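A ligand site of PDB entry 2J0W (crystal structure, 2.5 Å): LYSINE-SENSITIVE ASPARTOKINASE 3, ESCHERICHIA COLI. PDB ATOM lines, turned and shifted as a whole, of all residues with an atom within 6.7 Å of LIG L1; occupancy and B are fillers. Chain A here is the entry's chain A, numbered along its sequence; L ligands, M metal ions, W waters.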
ATOM      1  N   LYS A   8      -8.655 -17.942 -13.487  1.00  0.00           N
ATOM      2  CA  LYS A   8      -9.800 -18.830 -13.382  1.00  0.00           C
ATOM      3  C   LYS A   8     -10.967 -18.389 -14.247  1.00  0.00           C
ATOM      4  O   LYS A   8     -11.330 -17.216 -14.279  1.00  0.00           O
ATOM      5  CB  LYS A   8     -10.247 -18.960 -11.918  1.00  0.00           C
ATOM      6  CG  LYS A   8     -11.397 -19.928 -11.680  1.00  0.00           C
ATOM      7  CD  LYS A   8     -12.763 -19.283 -11.871  1.00  0.00           C
ATOM      8  CE  LYS A   8     -13.867 -20.200 -11.354  1.00  0.00           C
ATOM      9  NZ  LYS A   8     -15.211 -19.564 -11.267  1.00  0.00           N
ATOM     10  N   GLY A  10     -15.013 -19.278 -15.332  1.00  0.00           N
ATOM     11  CA  GLY A  10     -16.242 -19.946 -14.958  1.00  0.00           C
ATOM     12  C   GLY A  10     -17.078 -20.457 -16.121  1.00  0.00           C
ATOM     13  O   GLY A  10     -16.660 -20.385 -17.278  1.00  0.00           O
ATOM     14  N   GLY A  11     -18.266 -20.955 -15.792  1.00  0.00           N
ATOM     15  CA  GLY A  11     -19.169 -21.506 -16.790  1.00  0.00           C
ATOM     16  C   GLY A  11     -19.324 -20.639 -18.029  1.00  0.00           C
ATOM     17  O   GLY A  11     -18.884 -21.025 -19.107  1.00  0.00           O
ATOM     18  N   LEU A  38     -10.198 -24.045 -15.095  1.00  0.00           N
ATOM     19  CA  LEU A  38     -11.491 -23.972 -15.765  1.00  0.00           C
ATOM     20  C   LEU A  38     -12.564 -24.741 -15.038  1.00  0.00           C
ATOM     21  O   LEU A  38     -12.302 -25.771 -14.432  1.00  0.00           O
ATOM     22  CB  LEU A  38     -11.401 -24.547 -17.167  1.00  0.00           C
ATOM     23  CG  LEU A  38     -10.466 -23.953 -18.215  1.00  0.00           C
ATOM     24  CD1 LEU A  38     -10.595 -24.777 -19.484  1.00  0.00           C
ATOM     25  CD2 LEU A  38     -10.829 -22.489 -18.473  1.00  0.00           C
ATOM     26  N   SER A  39     -13.780 -24.205 -15.098  1.00  0.00           N
ATOM     27  CA  SER A  39     -14.951 -24.858 -14.523  1.00  0.00           C
ATOM     28  C   SER A  39     -15.482 -25.518 -15.791  1.00  0.00           C
ATOM     29  O   SER A  39     -14.928 -25.319 -16.863  1.00  0.00           O
ATOM     30  CB  SER A  39     -15.992 -23.840 -14.045  1.00  0.00           C
ATOM     31  OG  SER A  39     -15.574 -23.081 -12.922  1.00  0.00           O
ATOM     32  N   ALA A  40     -16.556 -26.278 -15.665  1.00  0.00           N
ATOM     33  CA  ALA A  40     -17.129 -26.922 -16.842  1.00  0.00           C
ATOM     34  C   ALA A  40     -17.960 -25.854 -17.520  1.00  0.00           C
ATOM     35  O   ALA A  40     -18.323 -24.843 -16.914  1.00  0.00           O
ATOM     36  CB  ALA A  40     -17.996 -28.101 -16.418  1.00  0.00           C
ATOM     37  N   SER A  41     -18.285 -26.072 -18.782  1.00  0.00           N
ATOM     38  CA  SER A  41     -19.098 -25.114 -19.522  1.00  0.00           C
ATOM     39  C   SER A  41     -20.482 -24.905 -18.902  1.00  0.00           C
ATOM     40  O   SER A  41     -21.042 -25.823 -18.308  1.00  0.00           O
ATOM     41  CB  SER A  41     -19.232 -25.564 -20.980  1.00  0.00           C
ATOM     42  OG  SER A  41     -17.947 -25.699 -21.557  1.00  0.00           O
ATOM     43  N   ILE A  44     -23.392 -27.578 -17.851  1.00  0.00           N
ATOM     44  CA  ILE A  44     -22.897 -28.943 -17.695  1.00  0.00           C
ATOM     45  C   ILE A  44     -23.070 -29.506 -16.289  1.00  0.00           C
ATOM     46  O   ILE A  44     -23.697 -30.549 -16.102  1.00  0.00           O
ATOM     47  CB  ILE A  44     -21.408 -29.056 -18.117  1.00  0.00           C
ATOM     48  CG1 ILE A  44     -21.293 -28.901 -19.634  1.00  0.00           C
ATOM     49  CG2 ILE A  44     -20.834 -30.426 -17.746  1.00  0.00           C
ATOM     50  CD1 ILE A  44     -22.099 -29.947 -20.414  1.00  0.00           C
ATOM     51  N   THR A  45     -22.533 -28.809 -15.292  1.00  0.00           N
ATOM     52  CA  THR A  45     -22.631 -29.298 -13.920  1.00  0.00           C
ATOM     53  C   THR A  45     -24.055 -29.570 -13.469  1.00  0.00           C
ATOM     54  O   THR A  45     -24.302 -30.596 -12.827  1.00  0.00           O
ATOM     55  CB  THR A  45     -21.915 -28.357 -12.929  1.00  0.00           C
ATOM     56  OG1 THR A  45     -20.513 -28.344 -13.223  1.00  0.00           O
ATOM     57  CG2 THR A  45     -22.102 -28.826 -11.479  1.00  0.00           C
ATOM     58  N   ASN A  46     -24.994 -28.676 -13.789  1.00  0.00           N
ATOM     59  CA  ASN A  46     -26.391 -28.906 -13.388  1.00  0.00           C
ATOM     60  C   ASN A  46     -26.931 -30.148 -14.105  1.00  0.00           C
ATOM     61  O   ASN A  46     -27.645 -30.965 -13.508  1.00  0.00           O
ATOM     62  CB  ASN A  46     -27.300 -27.720 -13.733  1.00  0.00           C
ATOM     63  CG  ASN A  46     -26.908 -26.429 -13.002  1.00  0.00           C
ATOM     64  OD1 ASN A  46     -26.428 -26.444 -11.864  1.00  0.00           O
ATOM     65  ND2 ASN A  46     -27.148 -25.305 -13.669  1.00  0.00           N
ATOM     66  N   VAL A 115     -20.034 -36.004 -11.650  1.00  0.00           N
ATOM     67  CA  VAL A 115     -19.980 -34.576 -11.903  1.00  0.00           C
ATOM     68  C   VAL A 115     -18.588 -34.092 -12.261  1.00  0.00           C
ATOM     69  O   VAL A 115     -18.442 -33.099 -12.943  1.00  0.00           O
ATOM     70  CB  VAL A 115     -20.501 -33.758 -10.714  1.00  0.00           C
ATOM     71  CG1 VAL A 115     -20.107 -32.303 -10.887  1.00  0.00           C
ATOM     72  CG2 VAL A 115     -22.034 -33.862 -10.628  1.00  0.00           C
ATOM     73  N   GLU A 119     -15.613 -30.568 -15.792  1.00  0.00           N
ATOM     74  CA  GLU A 119     -14.350 -29.845 -15.894  1.00  0.00           C
ATOM     75  C   GLU A 119     -13.311 -30.671 -16.661  1.00  0.00           C
ATOM     76  O   GLU A 119     -12.346 -30.134 -17.175  1.00  0.00           O
ATOM     77  CB  GLU A 119     -13.812 -29.468 -14.508  1.00  0.00           C
ATOM     78  CG  GLU A 119     -14.736 -29.728 -13.325  1.00  0.00           C
ATOM     79  CD  GLU A 119     -16.014 -28.908 -13.340  1.00  0.00           C
ATOM     80  OE1 GLU A 119     -17.101 -29.520 -13.422  1.00  0.00           O
ATOM     81  OE2 GLU A 119     -15.945 -27.675 -13.265  1.00  0.00           O
ATOM     82  N   GLY A 183     -10.751 -26.924 -11.875  1.00  0.00           N
ATOM     83  CA  GLY A 183     -11.036 -26.567 -10.501  1.00  0.00           C
ATOM     84  C   GLY A 183     -12.216 -27.414 -10.041  1.00  0.00           C
ATOM     85  O   GLY A 183     -12.712 -28.230 -10.822  1.00  0.00           O
ATOM     86  N   PHE A 184     -12.647 -27.228  -8.791  1.00  0.00           N
ATOM     87  CA  PHE A 184     -13.796 -27.940  -8.241  1.00  0.00           C
ATOM     88  C   PHE A 184     -13.599 -29.409  -7.845  1.00  0.00           C
ATOM     89  O   PHE A 184     -14.288 -29.910  -6.936  1.00  0.00           O
ATOM     90  CB  PHE A 184     -14.953 -27.831  -9.233  1.00  0.00           C
ATOM     91  CG  PHE A 184     -16.197 -28.567  -8.832  1.00  0.00           C
ATOM     92  CD1 PHE A 184     -16.821 -28.292  -7.618  1.00  0.00           C
ATOM     93  CD2 PHE A 184     -16.815 -29.443  -9.725  1.00  0.00           C
ATOM     94  CE1 PHE A 184     -18.069 -28.862  -7.303  1.00  0.00           C
ATOM     95  CE2 PHE A 184     -18.063 -30.028  -9.418  1.00  0.00           C
ATOM     96  CZ  PHE A 184     -18.696 -29.736  -8.210  1.00  0.00           C
ATOM     97  N   GLY A 197     -17.415 -28.673  -3.703  1.00  0.00           N
ATOM     98  CA  GLY A 197     -18.687 -28.025  -3.442  1.00  0.00           C
ATOM     99  C   GLY A 197     -18.954 -26.979  -4.506  1.00  0.00           C
ATOM    100  O   GLY A 197     -18.011 -26.408  -5.058  1.00  0.00           O
ATOM    101  N   ARG A 198     -20.232 -26.724  -4.801  1.00  0.00           N
ATOM    102  CA  ARG A 198     -20.594 -25.759  -5.828  1.00  0.00           C
ATOM    103  C   ARG A 198     -19.746 -24.494  -5.776  1.00  0.00           C
ATOM    104  O   ARG A 198     -19.445 -23.976  -4.687  1.00  0.00           O
ATOM    105  CB  ARG A 198     -22.075 -25.375  -5.693  1.00  0.00           C
ATOM    106  CG  ARG A 198     -23.032 -26.559  -5.763  1.00  0.00           C
ATOM    107  CD  ARG A 198     -22.716 -27.495  -6.925  1.00  0.00           C
ATOM    108  NE  ARG A 198     -22.797 -26.842  -8.227  1.00  0.00           N
ATOM    109  CZ  ARG A 198     -23.869 -26.873  -9.024  1.00  0.00           C
ATOM    110  NH1 ARG A 198     -24.955 -27.530  -8.655  1.00  0.00           N
ATOM    111  NH2 ARG A 198     -23.834 -26.239 -10.193  1.00  0.00           N
ATOM    112  N   GLY A 199     -19.345 -23.984  -6.948  1.00  0.00           N
ATOM    113  CA  GLY A 199     -18.545 -22.777  -7.008  1.00  0.00           C
ATOM    114  C   GLY A 199     -17.104 -22.991  -6.580  1.00  0.00           C
ATOM    115  O   GLY A 199     -16.322 -22.053  -6.513  1.00  0.00           O
ATOM    116  N   GLY A 200     -16.778 -24.246  -6.318  1.00  0.00           N
ATOM    117  CA  GLY A 200     -15.449 -24.604  -5.872  1.00  0.00           C
ATOM    118  C   GLY A 200     -14.311 -24.320  -6.819  1.00  0.00           C
ATOM    119  O   GLY A 200     -13.142 -24.400  -6.426  1.00  0.00           O
ATOM    120  N   SER A 201     -14.613 -23.984  -8.066  1.00  0.00           N
ATOM    121  CA  SER A 201     -13.528 -23.691  -8.983  1.00  0.00           C
ATOM    122  C   SER A 201     -12.758 -22.437  -8.532  1.00  0.00           C
ATOM    123  O   SER A 201     -11.588 -22.288  -8.876  1.00  0.00           O
ATOM    124  CB  SER A 201     -14.046 -23.502 -10.413  1.00  0.00           C
ATOM    125  OG  SER A 201     -14.454 -24.744 -10.970  1.00  0.00           O
ATOM    126  N   ASP A 202     -13.407 -21.537  -7.779  1.00  0.00           N
ATOM    127  CA  ASP A 202     -12.741 -20.334  -7.288  1.00  0.00           C
ATOM    128  C   ASP A 202     -11.740 -20.764  -6.244  1.00  0.00           C
ATOM    129  O   ASP A 202     -10.577 -20.331  -6.229  1.00  0.00           O
ATOM    130  CB  ASP A 202     -13.715 -19.361  -6.594  1.00  0.00           C
ATOM    131  CG  ASP A 202     -14.667 -18.705  -7.554  1.00  0.00           C
ATOM    132  OD1 ASP A 202     -14.227 -18.307  -8.668  1.00  0.00           O
ATOM    133  OD2 ASP A 202     -15.859 -18.568  -7.181  1.00  0.00           O
ATOM    134  N   TYR A 203     -12.230 -21.630  -5.372  1.00  0.00           N
ATOM    135  CA  TYR A 203     -11.427 -22.135  -4.293  1.00  0.00           C
ATOM    136  C   TYR A 203     -10.172 -22.806  -4.858  1.00  0.00           C
ATOM    137  O   TYR A 203      -9.059 -22.558  -4.379  1.00  0.00           O
ATOM    138  CB  TYR A 203     -12.270 -23.118  -3.471  1.00  0.00           C
ATOM    139  CG  TYR A 203     -11.680 -23.485  -2.134  1.00  0.00           C
ATOM    140  CD1 TYR A 203     -10.699 -22.695  -1.530  1.00  0.00           C
ATOM    141  CD2 TYR A 203     -12.125 -24.623  -1.461  1.00  0.00           C
ATOM    142  CE1 TYR A 203     -10.183 -23.031  -0.287  1.00  0.00           C
ATOM    143  CE2 TYR A 203     -11.606 -24.968  -0.215  1.00  0.00           C
ATOM    144  CZ  TYR A 203     -10.637 -24.168   0.370  1.00  0.00           C
ATOM    145  OH  TYR A 203     -10.163 -24.478   1.612  1.00  0.00           O
HETATM  146  N1  LIG L   1     -18.424 -26.548 -11.996  1.00  0.00           N
HETATM  147  C1  LIG L   1     -18.840 -26.404 -10.599  1.00  0.00           C
HETATM  148  C2  LIG L   1     -20.261 -25.802 -10.619  1.00  0.00           C
HETATM  149  O1  LIG L   1     -20.856 -25.724 -11.719  1.00  0.00           O
HETATM  150  C3  LIG L   1     -17.794 -25.529  -9.837  1.00  0.00           C
HETATM  151  C4  LIG L   1     -17.705 -24.037 -10.242  1.00  0.00           C
HETATM  152  O2  LIG L   1     -18.481 -23.605 -11.152  1.00  0.00           O
HETATM  153  O3  LIG L   1     -16.850 -23.278  -9.645  1.00  0.00           O
HETATM  154  O4  LIG L   1     -20.759 -25.377  -9.517  1.00  0.00           O
HETATM  155  P1  LG2 L   2     -18.611 -18.022 -12.313  1.00  0.00           P
HETATM  156  O1  LG2 L   2     -17.775 -17.064 -13.068  1.00  0.00           O
HETATM  157  O2  LG2 L   2     -18.919 -19.274 -13.112  1.00  0.00           O
HETATM  158  O3  LG2 L   2     -17.963 -18.404 -10.936  1.00  0.00           O
HETATM  159  P2  LG2 L   2     -21.056 -17.332 -10.898  1.00  0.00           P
HETATM  160  O4  LG2 L   2     -22.444 -17.336 -11.431  1.00  0.00           O
HETATM  161  O5  LG2 L   2     -20.695 -18.449  -9.979  1.00  0.00           O
HETATM  162  O6  LG2 L   2     -20.012 -17.296 -12.078  1.00  0.00           O
HETATM  163  O7  LG2 L   2     -20.997 -15.882 -10.178  1.00  0.00           O
HETATM  164  C1  LG2 L   2     -21.013 -14.561 -10.789  1.00  0.00           C
HETATM  165  C2  LG2 L   2     -22.289 -13.875 -10.336  1.00  0.00           C
HETATM  166  O8  LG2 L   2     -22.485 -13.709  -8.899  1.00  0.00           O
HETATM  167  C3  LG2 L   2     -22.611 -12.508 -10.859  1.00  0.00           C
HETATM  168  O9  LG2 L   2     -22.907 -12.740 -12.250  1.00  0.00           O
HETATM  169  C4  LG2 L   2     -23.783 -12.125  -9.986  1.00  0.00           C
HETATM  170  O10 LG2 L   2     -24.993 -12.684 -10.466  1.00  0.00           O
HETATM  171  C5  LG2 L   2     -23.446 -12.694  -8.651  1.00  0.00           C
HETATM  172  N1  LG2 L   2     -23.066 -11.669  -7.558  1.00  0.00           N
HETATM  173  C6  LG2 L   2     -23.643 -11.716  -6.345  1.00  0.00           C
HETATM  174  N2  LG2 L   2     -23.243 -10.789  -5.492  1.00  0.00           N
HETATM  175  C7  LG2 L   2     -22.331 -10.107  -6.199  1.00  0.00           C
HETATM  176  C8  LG2 L   2     -21.543  -8.957  -5.821  1.00  0.00           C
HETATM  177  N3  LG2 L   2     -21.573  -8.403  -4.666  1.00  0.00           N
HETATM  178  N4  LG2 L   2     -20.691  -8.478  -6.842  1.00  0.00           N
HETATM  179  C9  LG2 L   2     -20.616  -9.058  -8.117  1.00  0.00           C
HETATM  180  N5  LG2 L   2     -21.369 -10.143  -8.468  1.00  0.00           N
HETATM  181  C10 LG2 L   2     -22.193 -10.617  -7.502  1.00  0.00           C
HETATM  182 MG    MG M   1     -18.463 -19.712  -9.338  1.00  0.00          MG
HETATM  183  O   HOH W   1     -17.229 -21.198 -11.913  1.00  0.00           O
HETATM  184  O   HOH W   2     -19.909 -21.000 -10.653  1.00  0.00           O
HETATM  185  O   HOH W   3     -16.928 -20.680  -8.772  1.00  0.00           O
HETATM  186  O   HOH W   4     -19.168 -24.217 -14.394  1.00  0.00           O
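NH2 of Arg 198 sits at hydrogen-bond distance from OD1 of Asn 46.
OG of Ser 39 sits at hydrogen-bond distance from OG of Ser 201.
The side-chain carboxylate (OE2) of Glu 119 is in hydrogen-bond range of the backbone NH (N) of Ala 40 (2.8 Å).
Water W3 lies within hydrogen-bond range of the backbone carbonyl oxygen of Gly 199 (2.7 Å), an oxygen (O3) of LIG L1 (2.7 Å), the side-chain carboxylate of Asp 202 (2.9 Å) and the side-chain amino group of Lys 8 (3.2 Å).
Water W1 lies within hydrogen-bond range of NZ of Lys 8 (2.7 Å), OG of Ser 39 (2.7 Å), O2 of LIG L1 (2.8 Å) and O2 of LG2 L2 (2.8 Å).
Water W2 bridges an oxygen (O5) of LG2 L2 (2.8 Å) and an oxygen (O2) of LIG L1 (3.0 Å).
Water W4 bridges the backbone carbonyl oxygen (O) of Ala 40 (2.7 Å) and an oxygen (O2) of LIG L1 (3.4 Å).
The guanidinium group (NE) of Arg 198 lies within salt-bridge range of an oxygen (O4) of LIG L1, 2.8 Å away.
An oxygen (O3) of LIG L1 sits at hydrogen-bond distance from the backbone NH (N) of Ser 201 (2.8 Å).
O3 of LIG L1 sits close to OG of Ser 201 (3.1 Å).
N1 of LIG L1 lies within salt-bridge range of OE2 of Glu 119 (3.0 Å).
N1 of LIG L1 is in hydrogen-bond range of OG1 of Thr 45.
The backbone NH (N) of Gly 199 sits at hydrogen-bond distance from an oxygen (O4) of LIG L1, at 3.2 Å.
An oxygen (O2) of LIG L1 is in hydrogen-bond range of the side-chain hydroxyl (OG) of Ser 39, at 3.4 Å.
An oxygen (O3) of LIG L1 is in hydrogen-bond range of the backbone NH of Gly 200 (3.5 Å).
The side-chain amino group (NZ) of Lys 8 sits close to an oxygen (O3) of LG2 L2, 3.0 Å away.
N of Gly 11 lies within hydrogen-bond range of O2 of LG2 L2 (3.2 Å).
Phe 184 touches LIG L1.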
